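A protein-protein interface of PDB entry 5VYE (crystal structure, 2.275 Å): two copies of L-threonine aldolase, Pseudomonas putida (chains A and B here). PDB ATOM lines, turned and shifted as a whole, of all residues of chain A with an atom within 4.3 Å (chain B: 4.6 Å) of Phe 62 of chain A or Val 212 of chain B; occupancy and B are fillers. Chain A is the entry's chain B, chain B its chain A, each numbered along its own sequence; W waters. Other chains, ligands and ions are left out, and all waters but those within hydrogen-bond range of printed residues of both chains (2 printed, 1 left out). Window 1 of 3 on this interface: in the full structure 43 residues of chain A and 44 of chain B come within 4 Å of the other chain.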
ATOM      1  N   ALA A  61     -18.513  -7.810  -3.464  1.00  0.00           N
ATOM      2  CA  ALA A  61     -17.455  -7.834  -4.451  1.00  0.00           C
ATOM      3  C   ALA A  61     -16.989  -9.263  -4.702  1.00  0.00           C
ATOM      4  O   ALA A  61     -17.365 -10.197  -3.987  1.00  0.00           O
ATOM      5  CB  ALA A  61     -16.277  -7.025  -3.960  1.00  0.00           C
ATOM      6  N   PHE A  62     -16.037  -9.417  -5.636  1.00  0.00           N
ATOM      7  CA  PHE A  62     -15.638 -10.768  -6.018  1.00  0.00           C
ATOM      8  C   PHE A  62     -14.563 -11.377  -5.134  1.00  0.00           C
ATOM      9  O   PHE A  62     -14.557 -12.604  -4.964  1.00  0.00           O
ATOM     10  CB  PHE A  62     -15.152 -10.812  -7.465  1.00  0.00           C
ATOM     11  CG  PHE A  62     -16.223 -10.591  -8.489  1.00  0.00           C
ATOM     12  CD1 PHE A  62     -17.305 -11.458  -8.589  1.00  0.00           C
ATOM     13  CD2 PHE A  62     -16.125  -9.545  -9.403  1.00  0.00           C
ATOM     14  CE1 PHE A  62     -18.267 -11.278  -9.587  1.00  0.00           C
ATOM     15  CE2 PHE A  62     -17.106  -9.356 -10.388  1.00  0.00           C
ATOM     16  CZ  PHE A  62     -18.164 -10.207 -10.468  1.00  0.00           C
ATOM     17  N   ASN A  63     -13.646 -10.585  -4.576  1.00  0.00           N
ATOM     18  CA  ASN A  63     -12.596 -11.147  -3.716  1.00  0.00           C
ATOM     19  C   ASN A  63     -12.112 -10.090  -2.723  1.00  0.00           C
ATOM     20  O   ASN A  63     -12.500  -8.927  -2.776  1.00  0.00           O
ATOM     21  CB  ASN A  63     -11.428 -11.684  -4.550  1.00  0.00           C
ATOM     22  CG  ASN A  63     -10.559 -10.530  -5.199  1.00  0.00           C
ATOM     23  OD1 ASN A  63     -10.725  -9.365  -4.885  1.00  0.00           O
ATOM     24  ND2 ASN A  63      -9.704 -10.881  -6.125  1.00  0.00           N
ATOM     25  N   VAL A 212     -16.603 -17.826  -4.127  1.00  0.00           N
ATOM     26  CA  VAL A 212     -16.172 -16.495  -4.550  1.00  0.00           C
ATOM     27  C   VAL A 212     -16.960 -15.527  -3.701  1.00  0.00           C
ATOM     28  O   VAL A 212     -18.048 -15.856  -3.236  1.00  0.00           O
ATOM     29  CB  VAL A 212     -16.438 -16.202  -6.057  1.00  0.00           C
ATOM     30  CG1 VAL A 212     -15.523 -16.957  -6.968  1.00  0.00           C
ATOM     31  CG2 VAL A 212     -17.947 -16.437  -6.408  1.00  0.00           C
ATOM     32  N   GLY A 213     -16.465 -14.301  -3.586  1.00  0.00           N
ATOM     33  CA  GLY A 213     -17.283 -13.210  -3.099  1.00  0.00           C
ATOM     34  C   GLY A 213     -16.931 -12.780  -1.699  1.00  0.00           C
ATOM     35  O   GLY A 213     -16.627 -13.615  -0.829  1.00  0.00           O
ATOM     36  N   GLY A 235     -15.200  -2.997 -12.201  1.00  0.00           N
ATOM     37  CA  GLY A 235     -15.274  -4.378 -12.655  1.00  0.00           C
ATOM     38  C   GLY A 235     -15.670  -5.355 -11.579  1.00  0.00           C
ATOM     39  O   GLY A 235     -15.439  -6.559 -11.721  1.00  0.00           O
ATOM     40  N   GLN A 236     -16.305  -4.873 -10.517  1.00  0.00           N
ATOM     41  CA  GLN A 236     -16.592  -5.662  -9.331  1.00  0.00           C
ATOM     42  C   GLN A 236     -18.084  -5.886  -9.091  1.00  0.00           C
ATOM     43  O   GLN A 236     -18.460  -6.199  -7.970  1.00  0.00           O
ATOM     44  CB  GLN A 236     -15.967  -5.005  -8.102  1.00  0.00           C
ATOM     45  CG  GLN A 236     -14.488  -5.194  -8.116  1.00  0.00           C
ATOM     46  CD  GLN A 236     -14.125  -6.604  -7.800  1.00  0.00           C
ATOM     47  OE1 GLN A 236     -14.722  -7.242  -6.918  1.00  0.00           O
ATOM     48  NE2 GLN A 236     -13.156  -7.123  -8.536  1.00  0.00           N
ATOM     49  N   LEU A 237     -18.918  -5.786 -10.120  1.00  0.00           N
ATOM     50  CA  LEU A 237     -20.369  -5.954 -10.013  1.00  0.00           C
ATOM     51  C   LEU A 237     -20.793  -7.240 -10.694  1.00  0.00           C
ATOM     52  O   LEU A 237     -20.611  -7.394 -11.909  1.00  0.00           O
ATOM     53  CB  LEU A 237     -21.113  -4.803 -10.675  1.00  0.00           C
ATOM     54  CG  LEU A 237     -22.553  -4.660 -10.227  1.00  0.00           C
ATOM     55  CD1 LEU A 237     -22.536  -3.985  -8.839  1.00  0.00           C
ATOM     56  CD2 LEU A 237     -23.286  -3.829 -11.256  1.00  0.00           C
ATOM     57  N   ALA A 238     -21.368  -8.148  -9.921  1.00  0.00           N
ATOM     58  CA  ALA A 238     -21.800  -9.421 -10.440  1.00  0.00           C
ATOM     59  C   ALA A 238     -23.084  -9.254 -11.256  1.00  0.00           C
ATOM     60  O   ALA A 238     -24.053  -8.658 -10.797  1.00  0.00           O
ATOM     61  CB  ALA A 238     -22.031 -10.387  -9.295  1.00  0.00           C
ATOM     62  N   LEU A 244     -23.447 -14.655  -5.482  1.00  0.00           N
ATOM     63  CA  LEU A 244     -22.601 -14.114  -4.431  1.00  0.00           C
ATOM     64  C   LEU A 244     -23.357 -13.967  -3.122  1.00  0.00           C
ATOM     65  O   LEU A 244     -22.785 -14.143  -2.040  1.00  0.00           O
ATOM     66  CB  LEU A 244     -22.053 -12.728  -4.856  1.00  0.00           C
ATOM     67  CG  LEU A 244     -20.717 -12.730  -5.620  1.00  0.00           C
ATOM     68  CD1 LEU A 244     -20.855 -13.523  -6.873  1.00  0.00           C
ATOM     69  CD2 LEU A 244     -20.281 -11.305  -5.930  1.00  0.00           C
ATOM     70  N   PHE B  62     -13.465 -12.223 -13.476  1.00  0.00           N
ATOM     71  CA  PHE B  62     -14.746 -12.445 -12.805  1.00  0.00           C
ATOM     72  C   PHE B  62     -15.929 -12.073 -13.706  1.00  0.00           C
ATOM     73  O   PHE B  62     -16.982 -12.702 -13.620  1.00  0.00           O
ATOM     74  CB  PHE B  62     -14.824 -11.662 -11.487  1.00  0.00           C
ATOM     75  CG  PHE B  62     -13.945 -12.205 -10.376  1.00  0.00           C
ATOM     76  CD1 PHE B  62     -14.135 -13.484  -9.852  1.00  0.00           C
ATOM     77  CD2 PHE B  62     -12.929 -11.422  -9.845  1.00  0.00           C
ATOM     78  CE1 PHE B  62     -13.322 -13.965  -8.806  1.00  0.00           C
ATOM     79  CE2 PHE B  62     -12.129 -11.886  -8.842  1.00  0.00           C
ATOM     80  CZ  PHE B  62     -12.322 -13.160  -8.307  1.00  0.00           C
ATOM     81  N   ASN B  63     -15.813 -11.048 -14.562  1.00  0.00           N
ATOM     82  CA  ASN B  63     -16.953 -10.654 -15.388  1.00  0.00           C
ATOM     83  C   ASN B  63     -16.435  -9.981 -16.648  1.00  0.00           C
ATOM     84  O   ASN B  63     -15.237  -9.765 -16.799  1.00  0.00           O
ATOM     85  CB  ASN B  63     -17.915  -9.736 -14.617  1.00  0.00           C
ATOM     86  CG  ASN B  63     -17.335  -8.306 -14.346  1.00  0.00           C
ATOM     87  OD1 ASN B  63     -16.382  -7.861 -14.953  1.00  0.00           O
ATOM     88  ND2 ASN B  63     -17.949  -7.615 -13.436  1.00  0.00           N
ATOM     89  N   THR B 206     -20.651 -16.400 -18.457  1.00  0.00           N
ATOM     90  CA  THR B 206     -21.813 -16.090 -17.631  1.00  0.00           C
ATOM     91  C   THR B 206     -23.103 -16.061 -18.454  1.00  0.00           C
ATOM     92  O   THR B 206     -24.112 -16.636 -18.041  1.00  0.00           O
ATOM     93  CB  THR B 206     -21.602 -14.768 -16.893  1.00  0.00           C
ATOM     94  OG1 THR B 206     -20.495 -14.908 -15.988  1.00  0.00           O
ATOM     95  CG2 THR B 206     -22.780 -14.414 -16.058  1.00  0.00           C
ATOM     96  N   MET B 210     -23.276 -19.916 -16.936  1.00  0.00           N
ATOM     97  CA  MET B 210     -22.400 -20.026 -15.771  1.00  0.00           C
ATOM     98  C   MET B 210     -22.761 -18.993 -14.715  1.00  0.00           C
ATOM     99  O   MET B 210     -23.415 -17.982 -14.981  1.00  0.00           O
ATOM    100  CB  MET B 210     -20.923 -19.838 -16.125  1.00  0.00           C
ATOM    101  CG  MET B 210     -20.393 -20.708 -17.247  1.00  0.00           C
ATOM    102  SD  MET B 210     -18.612 -20.456 -17.417  1.00  0.00           S
ATOM    103  CE  MET B 210     -18.307 -21.546 -18.685  1.00  0.00           C
ATOM    104  N   ALA B 211     -22.284 -19.247 -13.505  1.00  0.00           N
ATOM    105  CA  ALA B 211     -22.576 -18.363 -12.387  1.00  0.00           C
ATOM    106  C   ALA B 211     -21.756 -17.081 -12.433  1.00  0.00           C
ATOM    107  O   ALA B 211     -22.256 -16.007 -12.089  1.00  0.00           O
ATOM    108  CB  ALA B 211     -22.309 -19.087 -11.078  1.00  0.00           C
ATOM    109  N   VAL B 212     -20.511 -17.179 -12.870  1.00  0.00           N
ATOM    110  CA  VAL B 212     -19.538 -16.126 -12.690  1.00  0.00           C
ATOM    111  C   VAL B 212     -18.410 -16.502 -13.624  1.00  0.00           C
ATOM    112  O   VAL B 212     -18.184 -17.698 -13.859  1.00  0.00           O
ATOM    113  CB  VAL B 212     -19.095 -16.006 -11.208  1.00  0.00           C
ATOM    114  CG1 VAL B 212     -18.317 -17.230 -10.715  1.00  0.00           C
ATOM    115  CG2 VAL B 212     -18.243 -14.796 -10.998  1.00  0.00           C
ATOM    116  N   GLY B 213     -17.781 -15.496 -14.234  1.00  0.00           N
ATOM    117  CA  GLY B 213     -16.472 -15.630 -14.848  1.00  0.00           C
ATOM    118  C   GLY B 213     -16.521 -15.496 -16.355  1.00  0.00           C
ATOM    119  O   GLY B 213     -17.545 -15.734 -17.008  1.00  0.00           O
ATOM    120  N   GLN B 236      -8.827  -9.076  -9.841  1.00  0.00           N
ATOM    121  CA  GLN B 236      -9.541  -9.969 -10.750  1.00  0.00           C
ATOM    122  C   GLN B 236      -8.985 -11.382 -10.725  1.00  0.00           C
ATOM    123  O   GLN B 236      -9.258 -12.164 -11.633  1.00  0.00           O
ATOM    124  CB  GLN B 236      -9.499  -9.424 -12.167  1.00  0.00           C
ATOM    125  CG  GLN B 236     -10.469  -8.278 -12.412  1.00  0.00           C
ATOM    126  CD  GLN B 236     -11.913  -8.738 -12.453  1.00  0.00           C
ATOM    127  OE1 GLN B 236     -12.241  -9.772 -13.022  1.00  0.00           O
ATOM    128  NE2 GLN B 236     -12.780  -7.968 -11.825  1.00  0.00           N
ATOM    129  N   LEU B 244     -14.078 -21.029 -11.412  1.00  0.00           N
ATOM    130  CA  LEU B 244     -14.251 -20.333 -12.683  1.00  0.00           C
ATOM    131  C   LEU B 244     -13.889 -21.185 -13.897  1.00  0.00           C
ATOM    132  O   LEU B 244     -14.472 -21.003 -14.995  1.00  0.00           O
ATOM    133  CB  LEU B 244     -13.375 -19.080 -12.740  1.00  0.00           C
ATOM    134  CG  LEU B 244     -13.974 -17.747 -12.240  1.00  0.00           C
ATOM    135  CD1 LEU B 244     -14.583 -17.865 -10.965  1.00  0.00           C
ATOM    136  CD2 LEU B 244     -12.888 -16.687 -12.115  1.00  0.00           C
HETATM  137  O   HOH W   1      -6.869  -9.968  -7.351  1.00  0.00           O
HETATM  138  O   HOH W   2     -11.677  -5.311 -10.418  1.00  0.00           O
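The side-chain amide nitrogen (ND2) of Asn 63 of chain B sits at hydrogen-bond distance from the backbone carbonyl oxygen (O) of Gly 235 of chain A (3.2 Å). ND2 of Asn 63 of chain B sits at hydrogen-bond distance from O of Leu 237 of chain A, at 3.1 Å. O of Gly 235 of chain A sits at hydrogen-bond distance from NE2 of Gln 236 of chain B (3.0 Å). The side-chain amide nitrogen of Gln 236 of chain A sits close to the side-chain amide nitrogen of Gln 236 of chain B (3.4 Å).
N of Gly 213 of chain B is in hydrogen-bond range of O of Phe 62 of chain B (3.0 Å). N of Phe 62 of chain B is in hydrogen-bond range of OE1 of Gln 236 of chain B, 2.8 Å away. O of Phe 62 of chain A lies within hydrogen-bond range of N of Gly 213 of chain A, 2.9 Å away. N of Phe 62 of chain A sits at hydrogen-bond distance from OE1 of Gln 236 of chain A, at 2.8 Å.
Phe 62 of chain A touches Phe 62 of chain B (CD2 to CB, 3.2 Å). CE2 of Phe 62 of chain A touches ND2 of Asn 63 of chain B, 3.6 Å away. CG2 of Val 212 of chain B touches CE1 of Phe 62 of chain A (3.8 Å). Asn 63 of chain A touches Phe 62 of chain B (ND2 to CE2, 3.8 Å).
Of the printed residues of chain B, Gln 236 of chain A touches Gln 236. Printed residues of chain A within 4 Å of Asn 63 of chain B: Phe 62 (3.6 Å), Gly 235 (3.2 Å) and Leu 237 (3.1 Å). Ala 211 of chain B touches none of the printed residues of chain A. Of chain A, only Phe 62 comes within 4 Å of Val 212 of chain B. Gly 213 of chain B touches none of the printed residues of chain A. The nearest printed residue of chain B that does not touch Gly 235 of chain A is Phe 62 of chain B (5.1 Å).
Printed residues of chain B that touch a printed residue of chain A: Phe 62, Asn 63, Val 212 and Gln 236. Along chain B the printed residues that touch a printed residue of chain A span positions 62 to 236. Printed residues of chain A that touch a printed residue of chain B: Phe 62, Asn 63, Gly 235, Gln 236 and Leu 237. Hydrophobic or aromatic side chains of chain A within 4 Å of the printed part of chain B: Phe 62. Among the printed residues, no Asp or Glu carboxylate lies within 4 Å of a Lys or Arg side-chain nitrogen of the other chain.
Phe 62 of chain A touches its own counterpart, Phe 62 of chain B. Phe 62 of chain A touches Asn 63 of chain B, and with the chains exchanged Asn 63 of chain A touches Phe 62 of chain B. Phe 62 of chain A touches Val 212 of chain B, but with the chains exchanged Val 212 of chain A does not touch Phe 62 of chain B (4.1 Å). Gln 236 of chain B touches its own counterpart, Gln 236 of chain A. 6 positions are printed for both chains.
Water W2 bridges NE2 of Gln 236 of chain A and NE2 of Gln 236 of chain B. Water W1 lies within hydrogen-bond range of the side-chain amide nitrogen (ND2) of Asn 63 of chain A (3.2 Å) and the backbone NH (N) of Gln 236 of chain B (3.3 Å).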
